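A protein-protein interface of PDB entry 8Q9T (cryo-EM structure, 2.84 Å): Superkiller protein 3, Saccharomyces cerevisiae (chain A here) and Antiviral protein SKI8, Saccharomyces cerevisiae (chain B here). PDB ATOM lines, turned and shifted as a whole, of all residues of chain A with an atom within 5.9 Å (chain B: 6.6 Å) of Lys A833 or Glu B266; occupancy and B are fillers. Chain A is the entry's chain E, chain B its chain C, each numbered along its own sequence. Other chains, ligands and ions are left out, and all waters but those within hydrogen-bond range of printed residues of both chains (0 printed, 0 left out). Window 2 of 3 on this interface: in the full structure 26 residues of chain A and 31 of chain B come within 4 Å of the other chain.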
ATOM      1  N   LEU A 791      14.705 -22.386  -2.082  1.00  0.00           N
ATOM      2  CA  LEU A 791      15.046 -22.464  -3.498  1.00  0.00           C
ATOM      3  C   LEU A 791      14.557 -23.770  -4.116  1.00  0.00           C
ATOM      4  O   LEU A 791      13.890 -23.764  -5.159  1.00  0.00           O
ATOM      5  CB  LEU A 791      16.555 -22.311  -3.684  1.00  0.00           C
ATOM      6  CG  LEU A 791      17.205 -21.112  -2.995  1.00  0.00           C
ATOM      7  CD1 LEU A 791      18.681 -21.046  -3.336  1.00  0.00           C
ATOM      8  CD2 LEU A 791      16.506 -19.818  -3.378  1.00  0.00           C
ATOM      9  N   CYS A 821       9.248 -17.466   2.282  1.00  0.00           N
ATOM     10  CA  CYS A 821      10.608 -17.131   1.878  1.00  0.00           C
ATOM     11  C   CYS A 821      10.888 -15.647   2.059  1.00  0.00           C
ATOM     12  O   CYS A 821      11.946 -15.268   2.577  1.00  0.00           O
ATOM     13  CB  CYS A 821      10.841 -17.545   0.427  1.00  0.00           C
ATOM     14  SG  CYS A 821      12.480 -17.146  -0.214  1.00  0.00           S
ATOM     15  N   LEU A 825      13.671 -13.972   4.562  1.00  0.00           N
ATOM     16  CA  LEU A 825      14.715 -13.093   4.043  1.00  0.00           C
ATOM     17  C   LEU A 825      14.707 -11.749   4.755  1.00  0.00           C
ATOM     18  O   LEU A 825      15.768 -11.181   5.033  1.00  0.00           O
ATOM     19  CB  LEU A 825      14.547 -12.902   2.538  1.00  0.00           C
ATOM     20  CG  LEU A 825      14.970 -14.086   1.674  1.00  0.00           C
ATOM     21  CD1 LEU A 825      14.544 -13.859   0.249  1.00  0.00           C
ATOM     22  CD2 LEU A 825      16.466 -14.294   1.754  1.00  0.00           C
ATOM     23  N   PHE A 830      18.313  -9.641   4.602  1.00  0.00           N
ATOM     24  CA  PHE A 830      18.346  -9.456   3.151  1.00  0.00           C
ATOM     25  C   PHE A 830      17.137  -8.615   2.758  1.00  0.00           C
ATOM     26  O   PHE A 830      16.127  -9.111   2.255  1.00  0.00           O
ATOM     27  CB  PHE A 830      18.349 -10.798   2.429  1.00  0.00           C
ATOM     28  CG  PHE A 830      19.586 -11.620   2.661  1.00  0.00           C
ATOM     29  CD1 PHE A 830      19.835 -12.201   3.891  1.00  0.00           C
ATOM     30  CD2 PHE A 830      20.491 -11.829   1.637  1.00  0.00           C
ATOM     31  CE1 PHE A 830      20.970 -12.959   4.098  1.00  0.00           C
ATOM     32  CE2 PHE A 830      21.623 -12.589   1.839  1.00  0.00           C
ATOM     33  CZ  PHE A 830      21.863 -13.153   3.070  1.00  0.00           C
ATOM     34  N   LEU A 831      17.247  -7.310   2.994  1.00  0.00           N
ATOM     35  CA  LEU A 831      16.112  -6.415   2.814  1.00  0.00           C
ATOM     36  C   LEU A 831      15.799  -6.120   1.354  1.00  0.00           C
ATOM     37  O   LEU A 831      14.703  -5.633   1.061  1.00  0.00           O
ATOM     38  CB  LEU A 831      16.358  -5.099   3.556  1.00  0.00           C
ATOM     39  CG  LEU A 831      16.494  -5.180   5.076  1.00  0.00           C
ATOM     40  CD1 LEU A 831      16.371  -3.804   5.690  1.00  0.00           C
ATOM     41  CD2 LEU A 831      15.459  -6.117   5.662  1.00  0.00           C
ATOM     42  N   LEU A 832      16.724  -6.392   0.435  1.00  0.00           N
ATOM     43  CA  LEU A 832      16.506  -6.062  -0.969  1.00  0.00           C
ATOM     44  C   LEU A 832      15.871  -7.197  -1.759  1.00  0.00           C
ATOM     45  O   LEU A 832      15.098  -6.936  -2.687  1.00  0.00           O
ATOM     46  CB  LEU A 832      17.828  -5.660  -1.627  1.00  0.00           C
ATOM     47  CG  LEU A 832      18.298  -4.224  -1.398  1.00  0.00           C
ATOM     48  CD1 LEU A 832      19.478  -3.904  -2.295  1.00  0.00           C
ATOM     49  CD2 LEU A 832      17.163  -3.241  -1.630  1.00  0.00           C
ATOM     50  N   LYS A 833      16.184  -8.447  -1.423  1.00  0.00           N
ATOM     51  CA  LYS A 833      15.565  -9.587  -2.089  1.00  0.00           C
ATOM     52  C   LYS A 833      14.130  -9.801  -1.626  1.00  0.00           C
ATOM     53  O   LYS A 833      13.288 -10.290  -2.399  1.00  0.00           O
ATOM     54  CB  LYS A 833      16.396 -10.843  -1.829  1.00  0.00           C
ATOM     55  CG  LYS A 833      16.008 -12.041  -2.666  1.00  0.00           C
ATOM     56  CD  LYS A 833      17.177 -12.991  -2.818  1.00  0.00           C
ATOM     57  CE  LYS A 833      16.849 -14.119  -3.778  1.00  0.00           C
ATOM     58  NZ  LYS A 833      16.213 -15.270  -3.083  1.00  0.00           N
ATOM     59  N   SER A 834      13.843  -9.437  -0.375  1.00  0.00           N
ATOM     60  CA  SER A 834      12.529  -9.680   0.202  1.00  0.00           C
ATOM     61  C   SER A 834      11.449  -8.887  -0.524  1.00  0.00           C
ATOM     62  O   SER A 834      10.344  -9.390  -0.739  1.00  0.00           O
ATOM     63  CB  SER A 834      12.553  -9.339   1.690  1.00  0.00           C
ATOM     64  OG  SER A 834      11.290  -9.548   2.287  1.00  0.00           O
ATOM     65  N   VAL A 835      11.751  -7.648  -0.913  1.00  0.00           N
ATOM     66  CA  VAL A 835      10.763  -6.827  -1.611  1.00  0.00           C
ATOM     67  C   VAL A 835      10.441  -7.412  -2.983  1.00  0.00           C
ATOM     68  O   VAL A 835       9.277  -7.443  -3.405  1.00  0.00           O
ATOM     69  CB  VAL A 835      11.262  -5.374  -1.711  1.00  0.00           C
ATOM     70  CG1 VAL A 835      10.455  -4.601  -2.737  1.00  0.00           C
ATOM     71  CG2 VAL A 835      11.176  -4.698  -0.360  1.00  0.00           C
ATOM     72  N   SER A 836      11.460  -7.883  -3.703  1.00  0.00           N
ATOM     73  CA  SER A 836      11.219  -8.485  -5.009  1.00  0.00           C
ATOM     74  C   SER A 836      10.393  -9.759  -4.887  1.00  0.00           C
ATOM     75  O   SER A 836       9.474  -9.995  -5.685  1.00  0.00           O
ATOM     76  CB  SER A 836      12.550  -8.768  -5.706  1.00  0.00           C
ATOM     77  OG  SER A 836      13.248  -9.817  -5.062  1.00  0.00           O
ATOM     78  N   ILE A 837      10.695 -10.590  -3.886  1.00  0.00           N
ATOM     79  CA  ILE A 837       9.892 -11.795  -3.700  1.00  0.00           C
ATOM     80  C   ILE A 837       8.468 -11.444  -3.275  1.00  0.00           C
ATOM     81  O   ILE A 837       7.513 -12.138  -3.645  1.00  0.00           O
ATOM     82  CB  ILE A 837      10.583 -12.746  -2.709  1.00  0.00           C
ATOM     83  CG1 ILE A 837      11.921 -13.195  -3.289  1.00  0.00           C
ATOM     84  CG2 ILE A 837       9.715 -13.953  -2.422  1.00  0.00           C
ATOM     85  CD1 ILE A 837      12.511 -14.391  -2.607  1.00  0.00           C
ATOM     86  N   ALA A 838       8.293 -10.361  -2.514  1.00  0.00           N
ATOM     87  CA  ALA A 838       6.951  -9.899  -2.174  1.00  0.00           C
ATOM     88  C   ALA A 838       6.172  -9.495  -3.419  1.00  0.00           C
ATOM     89  O   ALA A 838       4.981  -9.811  -3.551  1.00  0.00           O
ATOM     90  CB  ALA A 838       7.039  -8.729  -1.197  1.00  0.00           C
ATOM     91  N   LEU B 199      29.508 -13.474 -14.124  1.00  0.00           N
ATOM     92  CA  LEU B 199      29.862 -12.211 -13.496  1.00  0.00           C
ATOM     93  C   LEU B 199      31.371 -12.136 -13.325  1.00  0.00           C
ATOM     94  O   LEU B 199      32.044 -13.157 -13.173  1.00  0.00           O
ATOM     95  CB  LEU B 199      29.179 -12.041 -12.135  1.00  0.00           C
ATOM     96  CG  LEU B 199      27.652 -11.986 -12.115  1.00  0.00           C
ATOM     97  CD1 LEU B 199      27.146 -12.073 -10.690  1.00  0.00           C
ATOM     98  CD2 LEU B 199      27.155 -10.720 -12.783  1.00  0.00           C
ATOM     99  N   TYR B 221      27.579  -3.282 -10.404  1.00  0.00           N
ATOM    100  CA  TYR B 221      27.670  -2.713  -9.071  1.00  0.00           C
ATOM    101  C   TYR B 221      29.067  -2.161  -8.849  1.00  0.00           C
ATOM    102  O   TYR B 221      30.014  -2.492  -9.564  1.00  0.00           O
ATOM    103  CB  TYR B 221      27.345  -3.746  -7.984  1.00  0.00           C
ATOM    104  CG  TYR B 221      26.035  -4.457  -8.200  1.00  0.00           C
ATOM    105  CD1 TYR B 221      24.852  -3.744  -8.318  1.00  0.00           C
ATOM    106  CD2 TYR B 221      25.981  -5.839  -8.292  1.00  0.00           C
ATOM    107  CE1 TYR B 221      23.651  -4.387  -8.520  1.00  0.00           C
ATOM    108  CE2 TYR B 221      24.786  -6.491  -8.495  1.00  0.00           C
ATOM    109  CZ  TYR B 221      23.624  -5.762  -8.608  1.00  0.00           C
ATOM    110  OH  TYR B 221      22.425  -6.405  -8.810  1.00  0.00           O
ATOM    111  N   GLY B 245      27.419 -18.895  -6.567  1.00  0.00           N
ATOM    112  CA  GLY B 245      27.519 -17.658  -7.312  1.00  0.00           C
ATOM    113  C   GLY B 245      26.706 -16.504  -6.770  1.00  0.00           C
ATOM    114  O   GLY B 245      26.743 -15.417  -7.360  1.00  0.00           O
ATOM    115  N   SER B 246      25.980 -16.696  -5.671  1.00  0.00           N
ATOM    116  CA  SER B 246      25.109 -15.670  -5.114  1.00  0.00           C
ATOM    117  C   SER B 246      25.771 -14.850  -4.016  1.00  0.00           C
ATOM    118  O   SER B 246      25.117 -13.981  -3.433  1.00  0.00           O
ATOM    119  CB  SER B 246      23.829 -16.312  -4.575  1.00  0.00           C
ATOM    120  OG  SER B 246      24.130 -17.347  -3.659  1.00  0.00           O
ATOM    121  N   LEU B 247      27.045 -15.096  -3.725  1.00  0.00           N
ATOM    122  CA  LEU B 247      27.753 -14.412  -2.656  1.00  0.00           C
ATOM    123  C   LEU B 247      29.142 -14.029  -3.143  1.00  0.00           C
ATOM    124  O   LEU B 247      29.702 -14.676  -4.031  1.00  0.00           O
ATOM    125  CB  LEU B 247      27.859 -15.300  -1.413  1.00  0.00           C
ATOM    126  CG  LEU B 247      28.168 -14.636  -0.074  1.00  0.00           C
ATOM    127  CD1 LEU B 247      26.915 -14.019   0.495  1.00  0.00           C
ATOM    128  CD2 LEU B 247      28.760 -15.641   0.889  1.00  0.00           C
ATOM    129  N   GLU B 264      26.271  -9.542  -1.164  1.00  0.00           N
ATOM    130  CA  GLU B 264      25.264 -10.337  -1.853  1.00  0.00           C
ATOM    131  C   GLU B 264      25.176  -9.844  -3.292  1.00  0.00           C
ATOM    132  O   GLU B 264      24.853  -8.676  -3.531  1.00  0.00           O
ATOM    133  CB  GLU B 264      23.922 -10.226  -1.131  1.00  0.00           C
ATOM    134  CG  GLU B 264      22.862 -11.216  -1.555  1.00  0.00           C
ATOM    135  CD  GLU B 264      21.858 -10.620  -2.512  1.00  0.00           C
ATOM    136  OE1 GLU B 264      21.665  -9.386  -2.477  1.00  0.00           O
ATOM    137  OE2 GLU B 264      21.245 -11.385  -3.282  1.00  0.00           O
ATOM    138  N   THR B 265      25.465 -10.732  -4.246  1.00  0.00           N
ATOM    139  CA  THR B 265      25.741 -10.308  -5.615  1.00  0.00           C
ATOM    140  C   THR B 265      24.496 -10.120  -6.469  1.00  0.00           C
ATOM    141  O   THR B 265      24.597  -9.536  -7.553  1.00  0.00           O
ATOM    142  CB  THR B 265      26.660 -11.315  -6.308  1.00  0.00           C
ATOM    143  OG1 THR B 265      26.206 -12.646  -6.040  1.00  0.00           O
ATOM    144  CG2 THR B 265      28.080 -11.162  -5.813  1.00  0.00           C
ATOM    145  N   GLU B 266      23.333 -10.597  -6.029  1.00  0.00           N
ATOM    146  CA  GLU B 266      22.138 -10.460  -6.854  1.00  0.00           C
ATOM    147  C   GLU B 266      21.584  -9.042  -6.830  1.00  0.00           C
ATOM    148  O   GLU B 266      21.042  -8.579  -7.838  1.00  0.00           O
ATOM    149  CB  GLU B 266      21.069 -11.454  -6.407  1.00  0.00           C
ATOM    150  CG  GLU B 266      19.953 -11.652  -7.414  1.00  0.00           C
ATOM    151  CD  GLU B 266      19.112 -12.877  -7.117  1.00  0.00           C
ATOM    152  OE1 GLU B 266      19.407 -13.575  -6.125  1.00  0.00           O
ATOM    153  OE2 GLU B 266      18.156 -13.141  -7.877  1.00  0.00           O
ATOM    154  N   PHE B 267      21.704  -8.344  -5.701  1.00  0.00           N
ATOM    155  CA  PHE B 267      21.246  -6.970  -5.580  1.00  0.00           C
ATOM    156  C   PHE B 267      22.322  -6.007  -5.102  1.00  0.00           C
ATOM    157  O   PHE B 267      22.100  -4.793  -5.147  1.00  0.00           O
ATOM    158  CB  PHE B 267      20.041  -6.886  -4.629  1.00  0.00           C
ATOM    159  N   GLY B 268      23.466  -6.504  -4.642  1.00  0.00           N
ATOM    160  CA  GLY B 268      24.577  -5.648  -4.276  1.00  0.00           C
ATOM    161  C   GLY B 268      24.416  -4.945  -2.946  1.00  0.00           C
ATOM    162  O   GLY B 268      24.377  -3.713  -2.896  1.00  0.00           O
ATOM    163  N   GLU B 269      24.323  -5.707  -1.859  1.00  0.00           N
ATOM    164  CA  GLU B 269      24.160  -5.126  -0.537  1.00  0.00           C
ATOM    165  C   GLU B 269      25.080  -5.821   0.457  1.00  0.00           C
ATOM    166  O   GLU B 269      25.377  -7.011   0.332  1.00  0.00           O
ATOM    167  CB  GLU B 269      22.707  -5.208  -0.061  1.00  0.00           C
ATOM    168  CG  GLU B 269      22.174  -6.613   0.083  1.00  0.00           C
ATOM    169  CD  GLU B 269      20.833  -6.646   0.783  1.00  0.00           C
ATOM    170  OE1 GLU B 269      20.658  -5.900   1.769  1.00  0.00           O
ATOM    171  OE2 GLU B 269      19.953  -7.416   0.343  1.00  0.00           O
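The side-chain carboxylate (OE2) of Glu B269 lies close to the backbone NH (N) of Leu A832, 3.4 Å away.
The backbone carbonyl oxygen (O) of Leu A825 sits at hydrogen-bond distance from the backbone NH (N) of Phe A830 (3.0 Å).
The backbone carbonyl oxygen (O) of Glu B269 sits at hydrogen-bond distance from the backbone NH (N) of Glu B264 (3.1 Å).
The side-chain hydroxyl of Ser A836 lies within hydrogen-bond range of the backbone carbonyl oxygen of Lys A833 (2.7 Å).
OE1 of Glu B264 is in hydrogen-bond range of N of Phe B267, at 3.4 Å.
OH of Tyr B221 sits at hydrogen-bond distance from O of Glu B266.
Among the printed residues, pairs that only touch across the chains: Phe A830 with Glu B264, Phe A830 with Glu B269, Leu A831 with Glu B269, Leu A832 with Phe B267 and Lys A833 with Glu B266.
Lys A833 touches one residue of chain B.
Glu B266 touches one residue of chain A.
Of the printed residues of chain B, Leu A831 touches Glu B269 (3.8 Å).
Printed residues of chain B within 4 Å of Leu A832: Phe B267 and Glu B269.
Printed residues of chain A within 4 Å of Glu B269: Phe A830 (3.8 Å), Leu A831 (3.8 Å) and Leu A832 (3.4 Å).
Hydrophobic or aromatic side chains of chain A that line the printed part of chain B: Phe A830 and Leu A832.
Along chain B the printed residues that touch a printed residue of chain A span positions 264 to 269.
Among the printed residues, 6 pairs touch across the chains.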
